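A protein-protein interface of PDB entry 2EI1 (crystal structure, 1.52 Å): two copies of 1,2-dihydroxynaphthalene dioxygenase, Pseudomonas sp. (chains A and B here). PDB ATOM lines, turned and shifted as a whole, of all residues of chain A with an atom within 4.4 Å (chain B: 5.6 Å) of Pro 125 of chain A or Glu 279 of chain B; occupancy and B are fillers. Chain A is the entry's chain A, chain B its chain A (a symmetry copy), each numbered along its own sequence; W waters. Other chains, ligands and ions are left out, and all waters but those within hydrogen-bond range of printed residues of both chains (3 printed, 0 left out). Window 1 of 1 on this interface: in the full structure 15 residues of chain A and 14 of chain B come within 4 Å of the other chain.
Arg 71 of chain A touches Glu 277 of chain B (NH2 to CB, 3.6 Å). Ala 278 of chain B touches Trp 123 of chain A. Gly 124 of chain A touches Ala 278 of chain B. Gly 124 of chain A touches Tyr 280 of chain B. O of Ala 278 of chain B touches CD of Pro 125 of chain A, at 3.3 Å. O of Pro 125 of chain A touches CA of Glu 279 of chain B, at 3.5 Å. Tyr 280 of chain B touches Arg 126 of chain A. CG1 of Ile 127 of chain A touches CB of Glu 279 of chain B, 3.6 Å away. O of Ile 127 of chain A touches CD2 of Tyr 281 of chain B, at 3.3 Å.
Water W3 lies within hydrogen-bond range of the side-chain carboxylate of Glu 279 of chain B and the guanidinium group of Arg 71 of chain A. Water W2 lies within hydrogen-bond range of the backbone carbonyl oxygen (O) of Ala 278 of chain B (2.9 Å), the guanidinium group (NE) of Arg 71 of chain A (2.9 Å) and the backbone NH (N) of Gly 124 of chain A (2.9 Å). Water W1 bridges OH of Tyr 280 of chain B (3.0 Å) and NH1 of Arg 126 of chain A (3.4 Å).
O of Ala 278 of chain B lies within hydrogen-bond range of NH2 of Arg 71 of chain A. The side-chain hydroxyl of Tyr 280 of chain B sits at hydrogen-bond distance from the backbone carbonyl oxygen of Met 104 of chain A, 3.4 Å away. The backbone NH of Tyr 280 of chain B is in hydrogen-bond range of the backbone carbonyl oxygen of Pro 125 of chain A (2.9 Å). The backbone NH (N) of Ile 127 of chain A sits at hydrogen-bond distance from the backbone carbonyl oxygen (O) of Tyr 280 of chain B (2.9 Å).
The backbone carbonyl oxygen (O) of Met 104 of chain A lies within hydrogen-bond range of the backbone NH (N) of Arg 126 of chain A (3.3 Å). N of Tyr 281 of chain B sits at hydrogen-bond distance from O of Glu 177 of chain B, 2.8 Å away. The side-chain carboxylate (OE1) of Glu 279 of chain B sits at hydrogen-bond distance from the side-chain hydroxyl (OH) of Tyr 281 of chain B (2.5 Å).
Of the 10 printed residues of chain B, 5 touch a printed residue of chain A. Printed residues of chain B that touch a printed residue of chain A: Glu 277, Ala 278, Glu 279, Tyr 280 and Tyr 281. Hydrophobic or aromatic side chains of chain B within 4 Å of the printed part of chain A: Ala 278, Tyr 280 and Tyr 281. Hydrophobic or aromatic side chains of chain A that line the printed part of chain B: Met 104, Trp 123, Pro 125 and Ile 127. Among the printed residues, 13 pairs touch across the chains. Among the printed residues, no Asp or Glu carboxylate lies within 4 Å of a Lys or Arg side-chain nitrogen of the other chain.
No position is printed for both chains. Of the 13 pairs that touch across the chains among the printed residues, none has its exchanged pair printed and touching as well.
Trp 51 of chain A touches none of the printed residues of chain B. Of the printed residues of chain B, Trp 123 of chain A touches Ala 278. Of the printed residues of chain B, Gly 124 of chain A touches Ala 278 (3.4 Å) and Tyr 280 (3.3 Å). Pro 125 of chain A touches just these residues of chain B: Ala 278 (3.3 Å), Glu 279 (3.5 Å) and Tyr 280 (2.9 Å). Ile 275 of chain B touches none of the printed residues of chain A. Of the printed residues of chain A, Glu 277 of chain B touches Arg 71. Printed residues of chain A within 4 Å of Glu 279 of chain B: Pro 125 (3.5 Å) and Ile 127 (3.6 Å). Of the printed residues of chain A, Tyr 280 of chain B touches Met 104 (3.4 Å), Gly 124 (3.3 Å), Pro 125 (2.9 Å), Arg 126 (3.4 Å) and Ile 127 (2.9 Å). Printed residues of chain A within 4 Å of Tyr 281 of chain B: Ile 127. The nearest residue of chain B that does not touch Pro 125 of chain A is Tyr 281 of chain B (5.5 Å). The nearest printed residue of chain A that does not touch Glu 279 of chain B is Arg 71 of chain A (4.01 Å). The nearest printed residue of chain B that does not touch Gly 124 of chain A is Glu 279 of chain B (4.3 Å).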
ATOM      1  N   TRP A  51       4.582  16.894   1.072  1.00  0.00           N
ATOM      2  CA  TRP A  51       4.474  18.090   0.218  1.00  0.00           C
ATOM      3  C   TRP A  51       5.738  18.248  -0.624  1.00  0.00           C
ATOM      4  O   TRP A  51       6.835  17.923  -0.166  1.00  0.00           O
ATOM      5  CB  TRP A  51       4.269  19.343   1.067  1.00  0.00           C
ATOM      6  CG  TRP A  51       2.878  19.474   1.631  1.00  0.00           C
ATOM      7  CD1 TRP A  51       2.098  18.476   2.156  1.00  0.00           C
ATOM      8  CD2 TRP A  51       2.118  20.683   1.746  1.00  0.00           C
ATOM      9  NE1 TRP A  51       0.888  18.991   2.578  1.00  0.00           N
ATOM     10  CE2 TRP A  51       0.874  20.343   2.334  1.00  0.00           C
ATOM     11  CE3 TRP A  51       2.360  22.018   1.393  1.00  0.00           C
ATOM     12  CZ2 TRP A  51      -0.125  21.309   2.589  1.00  0.00           C
ATOM     13  CZ3 TRP A  51       1.375  22.985   1.647  1.00  0.00           C
ATOM     14  CH2 TRP A  51       0.146  22.617   2.243  1.00  0.00           C
ATOM     15  N   ARG A  71      -3.145  28.285   3.534  1.00  0.00           N
ATOM     16  CA  ARG A  71      -3.974  27.429   2.697  1.00  0.00           C
ATOM     17  C   ARG A  71      -5.454  27.591   3.037  1.00  0.00           C
ATOM     18  O   ARG A  71      -5.824  27.737   4.210  1.00  0.00           O
ATOM     19  CB  ARG A  71      -3.579  25.968   2.946  1.00  0.00           C
ATOM     20  CG  ARG A  71      -4.239  24.950   2.027  1.00  0.00           C
ATOM     21  CD  ARG A  71      -3.869  23.556   2.470  1.00  0.00           C
ATOM     22  NE  ARG A  71      -4.400  22.559   1.550  1.00  0.00           N
ATOM     23  CZ  ARG A  71      -4.338  21.248   1.771  1.00  0.00           C
ATOM     24  NH1 ARG A  71      -3.788  20.761   2.892  1.00  0.00           N
ATOM     25  NH2 ARG A  71      -4.843  20.406   0.863  1.00  0.00           N
ATOM     26  N   MET A 104       3.766  26.481  -7.061  1.00  0.00           N
ATOM     27  CA  MET A 104       3.256  25.100  -7.219  1.00  0.00           C
ATOM     28  C   MET A 104       1.915  24.885  -6.516  1.00  0.00           C
ATOM     29  O   MET A 104       1.715  23.912  -5.784  1.00  0.00           O
ATOM     30  CB  MET A 104       4.304  24.059  -6.798  1.00  0.00           C
ATOM     31  CG  MET A 104       5.613  24.226  -7.576  1.00  0.00           C
ATOM     32  SD  MET A 104       6.866  23.094  -6.989  1.00  0.00           S
ATOM     33  CE  MET A 104       8.329  23.723  -7.798  1.00  0.00           C
ATOM     34  N   PHE A 122      -3.772  30.571  -0.740  1.00  0.00           N
ATOM     35  CA  PHE A 122      -3.754  29.641  -1.862  1.00  0.00           C
ATOM     36  C   PHE A 122      -4.631  28.447  -1.609  1.00  0.00           C
ATOM     37  O   PHE A 122      -5.003  28.165  -0.466  1.00  0.00           O
ATOM     38  CB  PHE A 122      -2.320  29.161  -2.150  1.00  0.00           C
ATOM     39  CG  PHE A 122      -1.806  28.145  -1.161  1.00  0.00           C
ATOM     40  CD1 PHE A 122      -1.896  26.780  -1.430  1.00  0.00           C
ATOM     41  CD2 PHE A 122      -1.257  28.552   0.052  1.00  0.00           C
ATOM     42  CE1 PHE A 122      -1.429  25.836  -0.512  1.00  0.00           C
ATOM     43  CE2 PHE A 122      -0.795  27.611   0.983  1.00  0.00           C
ATOM     44  CZ  PHE A 122      -0.872  26.254   0.685  1.00  0.00           C
ATOM     45  N   TRP A 123      -4.938  27.728  -2.682  1.00  0.00           N
ATOM     46  CA  TRP A 123      -5.520  26.398  -2.543  1.00  0.00           C
ATOM     47  C   TRP A 123      -4.790  25.438  -3.468  1.00  0.00           C
ATOM     48  O   TRP A 123      -4.200  25.849  -4.479  1.00  0.00           O
ATOM     49  CB  TRP A 123      -7.039  26.378  -2.809  1.00  0.00           C
ATOM     50  CG  TRP A 123      -7.416  26.613  -4.250  1.00  0.00           C
ATOM     51  CD1 TRP A 123      -7.532  27.824  -4.887  1.00  0.00           C
ATOM     52  CD2 TRP A 123      -7.735  25.617  -5.224  1.00  0.00           C
ATOM     53  NE1 TRP A 123      -7.886  27.637  -6.198  1.00  0.00           N
ATOM     54  CE2 TRP A 123      -8.020  26.297  -6.437  1.00  0.00           C
ATOM     55  CE3 TRP A 123      -7.794  24.225  -5.198  1.00  0.00           C
ATOM     56  CZ2 TRP A 123      -8.367  25.625  -7.612  1.00  0.00           C
ATOM     57  CZ3 TRP A 123      -8.155  23.546  -6.368  1.00  0.00           C
ATOM     58  CH2 TRP A 123      -8.428  24.255  -7.560  1.00  0.00           C
ATOM     59  N   GLY A 124      -4.822  24.161  -3.112  1.00  0.00           N
ATOM     60  CA  GLY A 124      -4.270  23.133  -3.993  1.00  0.00           C
ATOM     61  C   GLY A 124      -2.757  23.030  -4.020  1.00  0.00           C
ATOM     62  O   GLY A 124      -2.133  23.244  -5.061  1.00  0.00           O
ATOM     63  N   PRO A 125      -2.152  22.649  -2.886  1.00  0.00           N
ATOM     64  CA  PRO A 125      -0.710  22.421  -2.881  1.00  0.00           C
ATOM     65  C   PRO A 125      -0.348  21.168  -3.685  1.00  0.00           C
ATOM     66  O   PRO A 125      -1.175  20.254  -3.836  1.00  0.00           O
ATOM     67  CB  PRO A 125      -0.414  22.178  -1.397  1.00  0.00           C
ATOM     68  CG  PRO A 125      -1.707  21.565  -0.867  1.00  0.00           C
ATOM     69  CD  PRO A 125      -2.762  22.366  -1.572  1.00  0.00           C
ATOM     70  N   ARG A 126       0.890  21.139  -4.167  1.00  0.00           N
ATOM     71  CA  ARG A 126       1.468  19.975  -4.822  1.00  0.00           C
ATOM     72  C   ARG A 126       2.022  19.026  -3.768  1.00  0.00           C
ATOM     73  O   ARG A 126       2.875  19.403  -2.947  1.00  0.00           O
ATOM     74  CB  ARG A 126       2.598  20.405  -5.764  1.00  0.00           C
ATOM     75  CG  ARG A 126       3.261  19.219  -6.427  1.00  0.00           C
ATOM     76  CD  ARG A 126       4.376  19.639  -7.355  1.00  0.00           C
ATOM     77  NE  ARG A 126       5.289  18.519  -7.564  1.00  0.00           N
ATOM     78  CZ  ARG A 126       6.293  18.523  -8.434  1.00  0.00           C
ATOM     79  NH1 ARG A 126       6.488  19.572  -9.221  1.00  0.00           N
ATOM     80  NH2 ARG A 126       7.089  17.469  -8.530  1.00  0.00           N
ATOM     81  N   ILE A 127       1.523  17.795  -3.799  1.00  0.00           N
ATOM     82  CA  ILE A 127       1.945  16.744  -2.880  1.00  0.00           C
ATOM     83  C   ILE A 127       2.671  15.674  -3.679  1.00  0.00           C
ATOM     84  O   ILE A 127       2.120  15.139  -4.654  1.00  0.00           O
ATOM     85  CB  ILE A 127       0.740  16.105  -2.158  1.00  0.00           C
ATOM     86  CG1 ILE A 127      -0.217  17.171  -1.610  1.00  0.00           C
ATOM     87  CG2 ILE A 127       1.217  15.127  -1.069  1.00  0.00           C
ATOM     88  CD1 ILE A 127       0.380  18.125  -0.649  1.00  0.00           C
ATOM     89  N   VAL B 176      -9.208  19.708  -9.822  1.00  0.00           N
ATOM     90  CA  VAL B 176      -8.042  19.105 -10.455  1.00  0.00           C
ATOM     91  C   VAL B 176      -7.149  18.467  -9.388  1.00  0.00           C
ATOM     92  O   VAL B 176      -6.707  19.153  -8.454  1.00  0.00           O
ATOM     93  CB  VAL B 176      -7.251  20.173 -11.243  1.00  0.00           C
ATOM     94  CG1 VAL B 176      -5.887  19.644 -11.669  1.00  0.00           C
ATOM     95  CG2 VAL B 176      -8.069  20.645 -12.455  1.00  0.00           C
ATOM     96  N   GLU B 177      -6.900  17.161  -9.515  1.00  0.00           N
ATOM     97  CA  GLU B 177      -5.995  16.460  -8.595  1.00  0.00           C
ATOM     98  C   GLU B 177      -4.742  15.930  -9.263  1.00  0.00           C
ATOM     99  O   GLU B 177      -3.800  15.556  -8.580  1.00  0.00           O
ATOM    100  CB  GLU B 177      -6.713  15.326  -7.840  1.00  0.00           C
ATOM    101  CG  GLU B 177      -7.735  15.849  -6.831  1.00  0.00           C
ATOM    102  CD  GLU B 177      -8.503  14.768  -6.106  1.00  0.00           C
ATOM    103  OE1 GLU B 177      -8.309  13.563  -6.400  1.00  0.00           O
ATOM    104  OE2 GLU B 177      -9.321  15.144  -5.236  1.00  0.00           O
ATOM    105  N   ALA B 248      -2.080   8.129  -6.004  1.00  0.00           N
ATOM    106  CA  ALA B 248      -1.735   9.151  -5.013  1.00  0.00           C
ATOM    107  C   ALA B 248      -2.942   9.758  -4.309  1.00  0.00           C
ATOM    108  O   ALA B 248      -2.850  10.108  -3.123  1.00  0.00           O
ATOM    109  CB  ALA B 248      -0.891  10.238  -5.657  1.00  0.00           C
ATOM    110  N   LYS B 251      -5.083   6.188  -2.644  1.00  0.00           N
ATOM    111  CA  LYS B 251      -4.177   5.238  -1.976  1.00  0.00           C
ATOM    112  C   LYS B 251      -4.578   3.766  -2.239  1.00  0.00           C
ATOM    113  O   LYS B 251      -4.112   2.861  -1.546  1.00  0.00           O
ATOM    114  CB  LYS B 251      -4.077   5.511  -0.454  1.00  0.00           C
ATOM    115  CG  LYS B 251      -3.947   6.999  -0.007  1.00  0.00           C
ATOM    116  CD  LYS B 251      -2.761   7.697  -0.634  1.00  0.00           C
ATOM    117  CE  LYS B 251      -2.566   9.115  -0.057  1.00  0.00           C
ATOM    118  NZ  LYS B 251      -3.672  10.082  -0.385  1.00  0.00           N
ATOM    119  N   ILE B 275     -11.185  13.487   1.015  1.00  0.00           N
ATOM    120  CA  ILE B 275     -10.890  14.700   1.790  1.00  0.00           C
ATOM    121  C   ILE B 275     -11.408  15.945   1.108  1.00  0.00           C
ATOM    122  O   ILE B 275     -11.343  16.035  -0.113  1.00  0.00           O
ATOM    123  CB  ILE B 275      -9.398  14.853   2.117  1.00  0.00           C
ATOM    124  CG1 ILE B 275      -8.546  14.871   0.848  1.00  0.00           C
ATOM    125  CG2 ILE B 275      -8.931  13.749   3.064  1.00  0.00           C
ATOM    126  CD1 ILE B 275      -7.130  15.342   1.124  1.00  0.00           C
ATOM    127  N   GLU B 277     -10.173  18.943   1.480  1.00  0.00           N
ATOM    128  CA  GLU B 277      -9.061  19.862   1.192  1.00  0.00           C
ATOM    129  C   GLU B 277      -8.382  19.475  -0.119  1.00  0.00           C
ATOM    130  O   GLU B 277      -7.827  18.382  -0.247  1.00  0.00           O
ATOM    131  CB  GLU B 277      -8.048  19.893   2.342  1.00  0.00           C
ATOM    132  CG  GLU B 277      -8.631  20.266   3.714  1.00  0.00           C
ATOM    133  CD  GLU B 277      -9.421  19.141   4.377  1.00  0.00           C
ATOM    134  OE1 GLU B 277      -9.103  17.944   4.156  1.00  0.00           O
ATOM    135  OE2 GLU B 277     -10.370  19.465   5.132  1.00  0.00           O
ATOM    136  N   ALA B 278      -8.418  20.388  -1.082  1.00  0.00           N
ATOM    137  CA  ALA B 278      -7.882  20.120  -2.416  1.00  0.00           C
ATOM    138  C   ALA B 278      -6.361  20.011  -2.393  1.00  0.00           C
ATOM    139  O   ALA B 278      -5.673  20.874  -1.851  1.00  0.00           O
ATOM    140  CB  ALA B 278      -8.314  21.225  -3.374  1.00  0.00           C
ATOM    141  N   GLU B 279      -5.833  18.961  -3.002  1.00  0.00           N
ATOM    142  CA  GLU B 279      -4.397  18.907  -3.291  1.00  0.00           C
ATOM    143  C   GLU B 279      -4.214  18.313  -4.680  1.00  0.00           C
ATOM    144  O   GLU B 279      -5.179  17.790  -5.266  1.00  0.00           O
ATOM    145  CB  GLU B 279      -3.633  18.131  -2.215  1.00  0.00           C
ATOM    146  CG  GLU B 279      -4.111  16.720  -2.040  1.00  0.00           C
ATOM    147  CD  GLU B 279      -3.601  15.988  -0.749  1.00  0.00           C
ATOM    148  OE1 GLU B 279      -3.185  14.832  -0.880  1.00  0.00           O
ATOM    149  OE2 GLU B 279      -3.636  16.521   0.374  1.00  0.00           O
ATOM    150  N   TYR B 280      -3.003  18.405  -5.228  1.00  0.00           N
ATOM    151  CA  TYR B 280      -2.737  17.766  -6.520  1.00  0.00           C
ATOM    152  C   TYR B 280      -1.390  17.054  -6.558  1.00  0.00           C
ATOM    153  O   TYR B 280      -0.519  17.309  -5.727  1.00  0.00           O
ATOM    154  CB  TYR B 280      -2.870  18.753  -7.692  1.00  0.00           C
ATOM    155  CG  TYR B 280      -1.682  19.660  -7.954  1.00  0.00           C
ATOM    156  CD1 TYR B 280      -1.540  20.868  -7.264  1.00  0.00           C
ATOM    157  CD2 TYR B 280      -0.702  19.318  -8.889  1.00  0.00           C
ATOM    158  CE1 TYR B 280      -0.453  21.724  -7.510  1.00  0.00           C
ATOM    159  CE2 TYR B 280       0.385  20.168  -9.152  1.00  0.00           C
ATOM    160  CZ  TYR B 280       0.503  21.370  -8.457  1.00  0.00           C
ATOM    161  OH  TYR B 280       1.567  22.223  -8.700  1.00  0.00           O
ATOM    162  N   TYR B 281      -1.253  16.158  -7.538  1.00  0.00           N
ATOM    163  CA  TYR B 281      -0.079  15.306  -7.697  1.00  0.00           C
ATOM    164  C   TYR B 281       0.360  15.334  -9.145  1.00  0.00           C
ATOM    165  O   TYR B 281      -0.425  15.683 -10.040  1.00  0.00           O
ATOM    166  CB  TYR B 281      -0.428  13.858  -7.334  1.00  0.00           C
ATOM    167  CG  TYR B 281      -1.363  13.765  -6.160  1.00  0.00           C
ATOM    168  CD1 TYR B 281      -2.741  13.658  -6.352  1.00  0.00           C
ATOM    169  CD2 TYR B 281      -0.880  13.847  -4.857  1.00  0.00           C
ATOM    170  CE1 TYR B 281      -3.612  13.611  -5.267  1.00  0.00           C
ATOM    171  CE2 TYR B 281      -1.747  13.803  -3.762  1.00  0.00           C
ATOM    172  CZ  TYR B 281      -3.114  13.689  -3.984  1.00  0.00           C
ATOM    173  OH  TYR B 281      -3.988  13.635  -2.921  1.00  0.00           O
HETATM  174  O   HOH W   1       3.942  21.531 -10.422  1.00  0.00           O
HETATM  175  O   HOH W   2      -6.141  23.410  -0.614  1.00  0.00           O
HETATM  176  O   HOH W   3      -4.557  17.922   2.511  1.00  0.00           O
